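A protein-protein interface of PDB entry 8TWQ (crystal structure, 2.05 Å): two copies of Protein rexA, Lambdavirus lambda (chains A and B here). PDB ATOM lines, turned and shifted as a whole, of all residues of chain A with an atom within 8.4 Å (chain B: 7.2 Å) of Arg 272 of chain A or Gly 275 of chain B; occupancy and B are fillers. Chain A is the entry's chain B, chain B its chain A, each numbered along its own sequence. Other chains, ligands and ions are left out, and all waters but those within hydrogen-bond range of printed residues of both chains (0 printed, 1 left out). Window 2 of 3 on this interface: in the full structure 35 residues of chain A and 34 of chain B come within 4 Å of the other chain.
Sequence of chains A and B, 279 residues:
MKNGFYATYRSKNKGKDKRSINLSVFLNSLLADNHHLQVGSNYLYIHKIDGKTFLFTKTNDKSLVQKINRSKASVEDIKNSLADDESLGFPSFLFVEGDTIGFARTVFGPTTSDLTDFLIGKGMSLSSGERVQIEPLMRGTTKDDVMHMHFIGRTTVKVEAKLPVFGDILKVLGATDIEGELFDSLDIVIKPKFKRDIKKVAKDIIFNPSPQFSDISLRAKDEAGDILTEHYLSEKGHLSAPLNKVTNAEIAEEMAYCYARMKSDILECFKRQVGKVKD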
ATOM      1  N   LYS A  18     -23.553  36.221 -31.074  1.00  0.00           N
ATOM      2  CA  LYS A  18     -23.000  35.785 -32.349  1.00  0.00           C
ATOM      3  C   LYS A  18     -23.848  34.663 -32.930  1.00  0.00           C
ATOM      4  O   LYS A  18     -24.230  33.727 -32.225  1.00  0.00           O
ATOM      5  CB  LYS A  18     -21.562  35.317 -32.164  1.00  0.00           C
ATOM      6  CG  LYS A  18     -20.600  36.436 -31.869  1.00  0.00           C
ATOM      7  CD  LYS A  18     -19.178  35.916 -31.760  1.00  0.00           C
ATOM      8  CE  LYS A  18     -18.319  36.886 -30.955  1.00  0.00           C
ATOM      9  NZ  LYS A  18     -18.551  36.679 -29.500  1.00  0.00           N
ATOM     10  N   GLU A 135     -13.699  37.870 -39.024  1.00  0.00           N
ATOM     11  CA  GLU A 135     -12.657  38.089 -38.015  1.00  0.00           C
ATOM     12  C   GLU A 135     -11.394  37.314 -38.373  1.00  0.00           C
ATOM     13  O   GLU A 135     -11.431  36.071 -38.391  1.00  0.00           O
ATOM     14  CB  GLU A 135     -13.152  37.633 -36.646  1.00  0.00           C
ATOM     15  CG  GLU A 135     -13.539  38.736 -35.665  1.00  0.00           C
ATOM     16  CD  GLU A 135     -13.326  38.307 -34.208  1.00  0.00           C
ATOM     17  OE1 GLU A 135     -14.308  38.021 -33.470  1.00  0.00           O
ATOM     18  OE2 GLU A 135     -12.155  38.265 -33.786  1.00  0.00           O
ATOM     19  N   LEU A 137      -8.351  35.096 -37.916  1.00  0.00           N
ATOM     20  CA  LEU A 137      -7.835  34.175 -36.911  1.00  0.00           C
ATOM     21  C   LEU A 137      -6.328  33.936 -37.039  1.00  0.00           C
ATOM     22  O   LEU A 137      -5.583  34.070 -36.058  1.00  0.00           O
ATOM     23  CB  LEU A 137      -8.577  32.844 -37.006  1.00  0.00           C
ATOM     24  CG  LEU A 137     -10.071  32.819 -36.777  1.00  0.00           C
ATOM     25  CD1 LEU A 137     -10.530  31.414 -36.955  1.00  0.00           C
ATOM     26  CD2 LEU A 137     -10.350  33.296 -35.377  1.00  0.00           C
ATOM     27  N   ASP A 265      -5.348  23.999 -35.568  1.00  0.00           N
ATOM     28  CA  ASP A 265      -5.028  25.352 -35.137  1.00  0.00           C
ATOM     29  C   ASP A 265      -6.236  26.276 -35.286  1.00  0.00           C
ATOM     30  O   ASP A 265      -6.581  27.017 -34.356  1.00  0.00           O
ATOM     31  CB  ASP A 265      -3.836  25.881 -35.932  1.00  0.00           C
ATOM     32  CG  ASP A 265      -2.519  25.443 -35.353  1.00  0.00           C
ATOM     33  OD1 ASP A 265      -2.472  24.325 -34.789  1.00  0.00           O
ATOM     34  OD2 ASP A 265      -1.540  26.217 -35.461  1.00  0.00           O
ATOM     35  N   ILE A 266      -6.902  26.226 -36.452  1.00  0.00           N
ATOM     36  CA  ILE A 266      -8.033  27.120 -36.731  1.00  0.00           C
ATOM     37  C   ILE A 266      -9.039  27.083 -35.586  1.00  0.00           C
ATOM     38  O   ILE A 266      -9.416  28.119 -35.020  1.00  0.00           O
ATOM     39  CB  ILE A 266      -8.730  26.747 -38.062  1.00  0.00           C
ATOM     40  CG1 ILE A 266      -7.796  26.721 -39.284  1.00  0.00           C
ATOM     41  CG2 ILE A 266      -9.913  27.677 -38.321  1.00  0.00           C
ATOM     42  CD1 ILE A 266      -6.765  27.751 -39.309  1.00  0.00           C
ATOM     43  N   LEU A 267      -9.515  25.884 -35.251  1.00  0.00           N
ATOM     44  CA  LEU A 267     -10.586  25.790 -34.268  1.00  0.00           C
ATOM     45  C   LEU A 267     -10.099  26.202 -32.886  1.00  0.00           C
ATOM     46  O   LEU A 267     -10.887  26.736 -32.095  1.00  0.00           O
ATOM     47  CB  LEU A 267     -11.172  24.380 -34.267  1.00  0.00           C
ATOM     48  CG  LEU A 267     -11.855  24.126 -35.622  1.00  0.00           C
ATOM     49  CD1 LEU A 267     -12.192  22.654 -35.875  1.00  0.00           C
ATOM     50  CD2 LEU A 267     -13.090  25.027 -35.790  1.00  0.00           C
ATOM     51  N   GLU A 268      -8.810  25.973 -32.594  1.00  0.00           N
ATOM     52  CA  GLU A 268      -8.182  26.523 -31.397  1.00  0.00           C
ATOM     53  C   GLU A 268      -8.324  28.042 -31.373  1.00  0.00           C
ATOM     54  O   GLU A 268      -8.874  28.616 -30.425  1.00  0.00           O
ATOM     55  CB  GLU A 268      -6.707  26.118 -31.358  1.00  0.00           C
ATOM     56  CG  GLU A 268      -6.393  24.913 -30.488  1.00  0.00           C
ATOM     57  CD  GLU A 268      -4.883  24.713 -30.276  1.00  0.00           C
ATOM     58  OE1 GLU A 268      -4.227  24.046 -31.121  1.00  0.00           O
ATOM     59  OE2 GLU A 268      -4.353  25.228 -29.257  1.00  0.00           O
ATOM     60  N   CYS A 269      -7.826  28.706 -32.421  1.00  0.00           N
ATOM     61  CA  CYS A 269      -8.006  30.149 -32.580  1.00  0.00           C
ATOM     62  C   CYS A 269      -9.467  30.544 -32.449  1.00  0.00           C
ATOM     63  O   CYS A 269      -9.815  31.492 -31.733  1.00  0.00           O
ATOM     64  CB  CYS A 269      -7.485  30.589 -33.947  1.00  0.00           C
ATOM     65  SG  CYS A 269      -5.786  31.114 -33.980  1.00  0.00           S
ATOM     66  N   PHE A 270     -10.331  29.832 -33.168  1.00  0.00           N
ATOM     67  CA  PHE A 270     -11.747  30.155 -33.185  1.00  0.00           C
ATOM     68  C   PHE A 270     -12.304  30.242 -31.778  1.00  0.00           C
ATOM     69  O   PHE A 270     -12.980  31.212 -31.422  1.00  0.00           O
ATOM     70  CB  PHE A 270     -12.488  29.095 -33.991  1.00  0.00           C
ATOM     71  CG  PHE A 270     -13.900  29.443 -34.312  1.00  0.00           C
ATOM     72  CD1 PHE A 270     -14.865  29.475 -33.323  1.00  0.00           C
ATOM     73  CD2 PHE A 270     -14.269  29.721 -35.621  1.00  0.00           C
ATOM     74  CE1 PHE A 270     -16.167  29.794 -33.620  1.00  0.00           C
ATOM     75  CE2 PHE A 270     -15.585  30.030 -35.937  1.00  0.00           C
ATOM     76  CZ  PHE A 270     -16.537  30.068 -34.936  1.00  0.00           C
ATOM     77  N   LYS A 271     -12.033  29.231 -30.962  1.00  0.00           N
ATOM     78  CA  LYS A 271     -12.690  29.171 -29.667  1.00  0.00           C
ATOM     79  C   LYS A 271     -12.146  30.212 -28.706  1.00  0.00           C
ATOM     80  O   LYS A 271     -12.883  30.694 -27.845  1.00  0.00           O
ATOM     81  CB  LYS A 271     -12.572  27.765 -29.082  1.00  0.00           C
ATOM     82  CG  LYS A 271     -13.689  26.863 -29.595  1.00  0.00           C
ATOM     83  CD  LYS A 271     -13.318  25.390 -29.602  1.00  0.00           C
ATOM     84  CE  LYS A 271     -12.801  24.927 -28.240  1.00  0.00           C
ATOM     85  NZ  LYS A 271     -13.894  24.548 -27.267  1.00  0.00           N
ATOM     86  N   ARG A 272     -10.886  30.603 -28.849  1.00  0.00           N
ATOM     87  CA  ARG A 272     -10.370  31.634 -27.965  1.00  0.00           C
ATOM     88  C   ARG A 272     -10.847  33.012 -28.401  1.00  0.00           C
ATOM     89  O   ARG A 272     -11.506  33.721 -27.634  1.00  0.00           O
ATOM     90  CB  ARG A 272      -8.841  31.570 -27.911  1.00  0.00           C
ATOM     91  CG  ARG A 272      -8.213  32.548 -26.922  1.00  0.00           C
ATOM     92  CD  ARG A 272      -8.878  32.485 -25.528  1.00  0.00           C
ATOM     93  NE  ARG A 272      -9.192  31.113 -25.101  1.00  0.00           N
ATOM     94  CZ  ARG A 272     -10.124  30.784 -24.202  1.00  0.00           C
ATOM     95  NH1 ARG A 272     -10.863  31.728 -23.610  1.00  0.00           N
ATOM     96  NH2 ARG A 272     -10.326  29.503 -23.901  1.00  0.00           N
ATOM     97  N   GLN A 273     -10.551  33.389 -29.648  1.00  0.00           N
ATOM     98  CA  GLN A 273     -10.804  34.755 -30.103  1.00  0.00           C
ATOM     99  C   GLN A 273     -12.287  35.060 -30.203  1.00  0.00           C
ATOM    100  O   GLN A 273     -12.731  36.151 -29.813  1.00  0.00           O
ATOM    101  CB  GLN A 273     -10.181  34.991 -31.471  1.00  0.00           C
ATOM    102  CG  GLN A 273      -8.730  34.744 -31.553  1.00  0.00           C
ATOM    103  CD  GLN A 273      -8.221  35.251 -32.856  1.00  0.00           C
ATOM    104  OE1 GLN A 273      -8.850  36.129 -33.465  1.00  0.00           O
ATOM    105  NE2 GLN A 273      -7.098  34.698 -33.322  1.00  0.00           N
ATOM    106  N   VAL A 274     -13.053  34.133 -30.774  1.00  0.00           N
ATOM    107  CA  VAL A 274     -14.457  34.367 -31.088  1.00  0.00           C
ATOM    108  C   VAL A 274     -15.360  33.865 -29.975  1.00  0.00           C
ATOM    109  O   VAL A 274     -16.187  34.612 -29.448  1.00  0.00           O
ATOM    110  CB  VAL A 274     -14.802  33.710 -32.444  1.00  0.00           C
ATOM    111  CG1 VAL A 274     -16.287  33.713 -32.670  1.00  0.00           C
ATOM    112  CG2 VAL A 274     -14.086  34.429 -33.569  1.00  0.00           C
ATOM    113  N   GLY A 275     -15.202  32.613 -29.568  1.00  0.00           N
ATOM    114  CA  GLY A 275     -16.122  32.050 -28.608  1.00  0.00           C
ATOM    115  C   GLY A 275     -17.194  31.306 -29.366  1.00  0.00           C
ATOM    116  O   GLY A 275     -16.930  30.810 -30.463  1.00  0.00           O
ATOM    117  N   LYS A 276     -18.407  31.236 -28.841  1.00  0.00           N
ATOM    118  CA  LYS A 276     -19.402  30.402 -29.497  1.00  0.00           C
ATOM    119  C   LYS A 276     -20.177  31.190 -30.552  1.00  0.00           C
ATOM    120  O   LYS A 276     -20.318  32.415 -30.479  1.00  0.00           O
ATOM    121  CB  LYS A 276     -20.357  29.767 -28.479  1.00  0.00           C
ATOM    122  CG  LYS A 276     -19.635  28.950 -27.387  1.00  0.00           C
ATOM    123  CD  LYS A 276     -20.007  27.463 -27.413  1.00  0.00           C
ATOM    124  CE  LYS A 276     -18.903  26.594 -26.790  1.00  0.00           C
ATOM    125  NZ  LYS A 276     -18.266  25.614 -27.737  1.00  0.00           N
ATOM    126  N   LYS B  18     -20.461  28.449 -17.120  1.00  0.00           N
ATOM    127  CA  LYS B  18     -19.401  28.260 -16.138  1.00  0.00           C
ATOM    128  C   LYS B  18     -18.892  29.620 -15.677  1.00  0.00           C
ATOM    129  O   LYS B  18     -18.491  30.444 -16.504  1.00  0.00           O
ATOM    130  CB  LYS B  18     -18.253  27.421 -16.733  1.00  0.00           C
ATOM    131  CG  LYS B  18     -18.593  25.953 -16.947  1.00  0.00           C
ATOM    132  CD  LYS B  18     -17.413  25.163 -17.459  1.00  0.00           C
ATOM    133  CE  LYS B  18     -17.688  24.540 -18.804  1.00  0.00           C
ATOM    134  NZ  LYS B  18     -17.325  25.536 -19.859  1.00  0.00           N
ATOM    135  N   GLU B 135     -12.719  20.230 -11.390  1.00  0.00           N
ATOM    136  CA  GLU B 135     -12.601  19.267 -12.482  1.00  0.00           C
ATOM    137  C   GLU B 135     -11.147  18.888 -12.714  1.00  0.00           C
ATOM    138  O   GLU B 135     -10.329  19.767 -13.032  1.00  0.00           O
ATOM    139  CB  GLU B 135     -13.207  19.822 -13.773  1.00  0.00           C
ATOM    140  CG  GLU B 135     -13.206  18.780 -14.883  1.00  0.00           C
ATOM    141  CD  GLU B 135     -13.639  19.308 -16.233  1.00  0.00           C
ATOM    142  OE1 GLU B 135     -14.338  20.352 -16.299  1.00  0.00           O
ATOM    143  OE2 GLU B 135     -13.259  18.668 -17.241  1.00  0.00           O
ATOM    144  N   LEU B 137      -7.839  18.068 -14.517  1.00  0.00           N
ATOM    145  CA  LEU B 137      -7.240  18.313 -15.828  1.00  0.00           C
ATOM    146  C   LEU B 137      -6.065  17.404 -16.125  1.00  0.00           C
ATOM    147  O   LEU B 137      -5.771  17.143 -17.295  1.00  0.00           O
ATOM    148  CB  LEU B 137      -6.745  19.759 -15.938  1.00  0.00           C
ATOM    149  CG  LEU B 137      -7.740  20.880 -15.665  1.00  0.00           C
ATOM    150  CD1 LEU B 137      -6.989  22.199 -15.533  1.00  0.00           C
ATOM    151  CD2 LEU B 137      -8.791  20.938 -16.776  1.00  0.00           C
ATOM    152  N   LEU B 267      -3.096  25.075 -18.697  1.00  0.00           N
ATOM    153  CA  LEU B 267      -3.927  26.061 -19.378  1.00  0.00           C
ATOM    154  C   LEU B 267      -4.426  25.574 -20.737  1.00  0.00           C
ATOM    155  O   LEU B 267      -5.373  26.152 -21.284  1.00  0.00           O
ATOM    156  CB  LEU B 267      -3.150  27.372 -19.522  1.00  0.00           C
ATOM    157  CG  LEU B 267      -2.876  28.033 -18.163  1.00  0.00           C
ATOM    158  CD1 LEU B 267      -2.388  29.466 -18.307  1.00  0.00           C
ATOM    159  CD2 LEU B 267      -4.124  27.986 -17.284  1.00  0.00           C
ATOM    160  N   GLU B 268      -3.826  24.522 -21.288  1.00  0.00           N
ATOM    161  CA  GLU B 268      -4.339  23.980 -22.535  1.00  0.00           C
ATOM    162  C   GLU B 268      -5.331  22.854 -22.289  1.00  0.00           C
ATOM    163  O   GLU B 268      -6.374  22.799 -22.947  1.00  0.00           O
ATOM    164  CB  GLU B 268      -3.184  23.500 -23.411  1.00  0.00           C
ATOM    165  CG  GLU B 268      -2.590  24.614 -24.271  1.00  0.00           C
ATOM    166  CD  GLU B 268      -2.435  24.196 -25.732  1.00  0.00           C
ATOM    167  OE1 GLU B 268      -2.076  23.013 -25.957  1.00  0.00           O
ATOM    168  OE2 GLU B 268      -2.661  25.036 -26.648  1.00  0.00           O
ATOM    169  N   CYS B 269      -5.044  21.959 -21.340  1.00  0.00           N
ATOM    170  CA  CYS B 269      -6.052  20.979 -20.954  1.00  0.00           C
ATOM    171  C   CYS B 269      -7.295  21.677 -20.430  1.00  0.00           C
ATOM    172  O   CYS B 269      -8.410  21.168 -20.595  1.00  0.00           O
ATOM    173  CB  CYS B 269      -5.480  19.999 -19.924  1.00  0.00           C
ATOM    174  SG  CYS B 269      -4.633  18.605 -20.723  1.00  0.00           S
ATOM    175  N   PHE B 270      -7.120  22.857 -19.828  1.00  0.00           N
ATOM    176  CA  PHE B 270      -8.215  23.758 -19.500  1.00  0.00           C
ATOM    177  C   PHE B 270      -9.080  24.015 -20.725  1.00  0.00           C
ATOM    178  O   PHE B 270     -10.173  23.461 -20.851  1.00  0.00           O
ATOM    179  CB  PHE B 270      -7.669  25.083 -18.960  1.00  0.00           C
ATOM    180  CG  PHE B 270      -8.674  25.886 -18.180  1.00  0.00           C
ATOM    181  CD1 PHE B 270      -9.648  26.628 -18.829  1.00  0.00           C
ATOM    182  CD2 PHE B 270      -8.642  25.898 -16.797  1.00  0.00           C
ATOM    183  CE1 PHE B 270     -10.577  27.360 -18.114  1.00  0.00           C
ATOM    184  CE2 PHE B 270      -9.560  26.629 -16.068  1.00  0.00           C
ATOM    185  CZ  PHE B 270     -10.528  27.368 -16.724  1.00  0.00           C
ATOM    186  N   LYS B 271      -8.576  24.836 -21.646  1.00  0.00           N
ATOM    187  CA  LYS B 271      -9.372  25.253 -22.794  1.00  0.00           C
ATOM    188  C   LYS B 271      -9.933  24.071 -23.582  1.00  0.00           C
ATOM    189  O   LYS B 271     -11.019  24.174 -24.169  1.00  0.00           O
ATOM    190  CB  LYS B 271      -8.522  26.168 -23.670  1.00  0.00           C
ATOM    191  CG  LYS B 271      -8.040  27.383 -22.885  1.00  0.00           C
ATOM    192  CD  LYS B 271      -7.049  28.247 -23.652  1.00  0.00           C
ATOM    193  CE  LYS B 271      -6.555  29.401 -22.774  1.00  0.00           C
ATOM    194  NZ  LYS B 271      -5.210  29.936 -23.191  1.00  0.00           N
ATOM    195  N   ARG B 272      -9.240  22.932 -23.586  1.00  0.00           N
ATOM    196  CA  ARG B 272      -9.805  21.751 -24.228  1.00  0.00           C
ATOM    197  C   ARG B 272     -10.924  21.151 -23.383  1.00  0.00           C
ATOM    198  O   ARG B 272     -12.055  20.997 -23.858  1.00  0.00           O
ATOM    199  CB  ARG B 272      -8.714  20.708 -24.517  1.00  0.00           C
ATOM    200  CG  ARG B 272      -9.244  19.473 -25.284  1.00  0.00           C
ATOM    201  CD  ARG B 272      -8.179  18.428 -25.656  1.00  0.00           C
ATOM    202  NE  ARG B 272      -8.763  17.083 -25.742  1.00  0.00           N
ATOM    203  CZ  ARG B 272      -9.000  16.425 -26.878  1.00  0.00           C
ATOM    204  NH1 ARG B 272      -8.720  16.976 -28.055  1.00  0.00           N
ATOM    205  NH2 ARG B 272      -9.530  15.209 -26.839  1.00  0.00           N
ATOM    206  N   GLN B 273     -10.638  20.820 -22.117  1.00  0.00           N
ATOM    207  CA  GLN B 273     -11.573  20.008 -21.334  1.00  0.00           C
ATOM    208  C   GLN B 273     -12.729  20.811 -20.725  1.00  0.00           C
ATOM    209  O   GLN B 273     -13.783  20.230 -20.432  1.00  0.00           O
ATOM    210  CB  GLN B 273     -10.838  19.270 -20.212  1.00  0.00           C
ATOM    211  CG  GLN B 273      -9.707  18.347 -20.641  1.00  0.00           C
ATOM    212  CD  GLN B 273      -9.171  17.520 -19.464  1.00  0.00           C
ATOM    213  OE1 GLN B 273      -9.875  17.321 -18.468  1.00  0.00           O
ATOM    214  NE2 GLN B 273      -7.927  17.034 -19.577  1.00  0.00           N
ATOM    215  N   VAL B 274     -12.565  22.118 -20.500  1.00  0.00           N
ATOM    216  CA  VAL B 274     -13.580  22.893 -19.786  1.00  0.00           C
ATOM    217  C   VAL B 274     -13.919  24.136 -20.593  1.00  0.00           C
ATOM    218  O   VAL B 274     -15.064  24.600 -20.591  1.00  0.00           O
ATOM    219  CB  VAL B 274     -13.118  23.259 -18.358  1.00  0.00           C
ATOM    220  CG1 VAL B 274     -11.738  23.873 -18.361  1.00  0.00           C
ATOM    221  CG2 VAL B 274     -14.085  24.224 -17.706  1.00  0.00           C
ATOM    222  N   GLY B 275     -12.939  24.680 -21.278  1.00  0.00           N
ATOM    223  CA  GLY B 275     -13.180  25.790 -22.193  1.00  0.00           C
ATOM    224  C   GLY B 275     -13.075  27.137 -21.492  1.00  0.00           C
ATOM    225  O   GLY B 275     -11.981  27.529 -21.042  1.00  0.00           O
ATOM    226  N   LYS B 276     -14.205  27.846 -21.408  1.00  0.00           N
ATOM    227  CA  LYS B 276     -14.252  29.234 -20.966  1.00  0.00           C
ATOM    228  C   LYS B 276     -15.060  29.352 -19.683  1.00  0.00           C
ATOM    229  O   LYS B 276     -16.180  28.834 -19.589  1.00  0.00           O
ATOM    230  CB  LYS B 276     -14.841  30.147 -22.048  1.00  0.00           C
ATOM    231  CG  LYS B 276     -16.137  29.638 -22.680  1.00  0.00           C
ATOM    232  CD  LYS B 276     -16.233  30.070 -24.156  1.00  0.00           C
ATOM    233  CE  LYS B 276     -17.657  30.464 -24.566  1.00  0.00           C
ATOM    234  NZ  LYS B 276     -17.682  31.525 -25.621  1.00  0.00           N
ATOM    235  N   VAL B 277     -14.482  30.038 -18.706  1.00  0.00           N
ATOM    236  CA  VAL B 277     -15.105  30.288 -17.420  1.00  0.00           C
ATOM    237  C   VAL B 277     -15.195  31.806 -17.282  1.00  0.00           C
ATOM    238  O   VAL B 277     -14.163  32.488 -17.196  1.00  0.00           O
ATOM    239  CB  VAL B 277     -14.305  29.652 -16.272  1.00  0.00           C
ATOM    240  CG1 VAL B 277     -14.839  30.095 -14.931  1.00  0.00           C
ATOM    241  CG2 VAL B 277     -14.315  28.126 -16.397  1.00  0.00           C
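Arg 272 of chain A touches just these residues of chain B: Lys 271 and Gly 275. Gly 275 of chain B touches just one residue of chain A: Arg 272. No residue of chain A comes within 4 Å of Val 274 of chain B. Printed residues of chain B within 4 Å of Gly 275 of chain A: Lys 276. Printed residues of chain A within 4 Å of Lys 271 of chain B: Arg 272 (3.3 Å). Of the printed residues of chain B, Glu 268 of chain A touches Glu 268. Glu 135 of chain A touches none of the printed residues of chain B. Lys 271 of chain A touches none of the printed residues of chain B. The nearest residue of chain B that does not touch Arg 272 of chain A is Lys 276 of chain B (4.6 Å). The nearest printed residue of chain B that does not touch Glu 268 of chain A is Lys 271 of chain B (6.9 Å).
Glu 268 of chain B touches its own counterpart, Glu 268 of chain A. Arg 272 of chain A touches Lys 271 of chain B, but with the chains exchanged Lys 271 of chain A does not touch Arg 272 of chain B (5.3 Å). Arg 272 of chain A touches Gly 275 of chain B, but with the chains exchanged Gly 275 of chain A does not touch Arg 272 of chain B (12.5 Å). Lys 276 of chain A touches its own counterpart, Lys 276 of chain B. Positions printed for both chains: 18, 135, 137, 267, 268, 269, 270, 271, 272, 273, 274, 275 and 276.
The side-chain carboxylate (OE2) of Glu 268 of chain A sits close to the side-chain carboxylate (OE2) of Glu 268 of chain B (3.1 Å). The side-chain amino group of Lys 276 of chain B lies close to the backbone NH of Lys 276 of chain A.
Lys 271 of chain B touches Arg 272 of chain A (CG to NH2, 3.3 Å). NH2 of Arg 272 of chain A touches O of Gly 275 of chain B, at 3.8 Å. Gly 275 of chain A touches Lys 276 of chain B (CA to NZ, 3.4 Å).
O of Phe 270 of chain B is in hydrogen-bond range of N of Gly 275 of chain B, at 3.1 Å. The backbone carbonyl oxygen (O) of Phe 270 of chain A lies within hydrogen-bond range of the backbone NH (N) of Gly 275 of chain A.
Of the 14 printed residues of chain B, 4 touch a printed residue of chain A. Printed residues of chain B that touch a printed residue of chain A: Glu 268, Lys 271, Gly 275 and Lys 276. Of the 15 printed residues of chain A, 4 touch a printed residue of chain B. Printed residues of chain A that touch a printed residue of chain B: Glu 268, Arg 272, Gly 275 and Lys 276. Among the printed residues, 5 pairs touch across the chains. Among the printed residues, no Asp or Glu carboxylate lies within 4 Å of a Lys or Arg side-chain nitrogen of the other chain.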
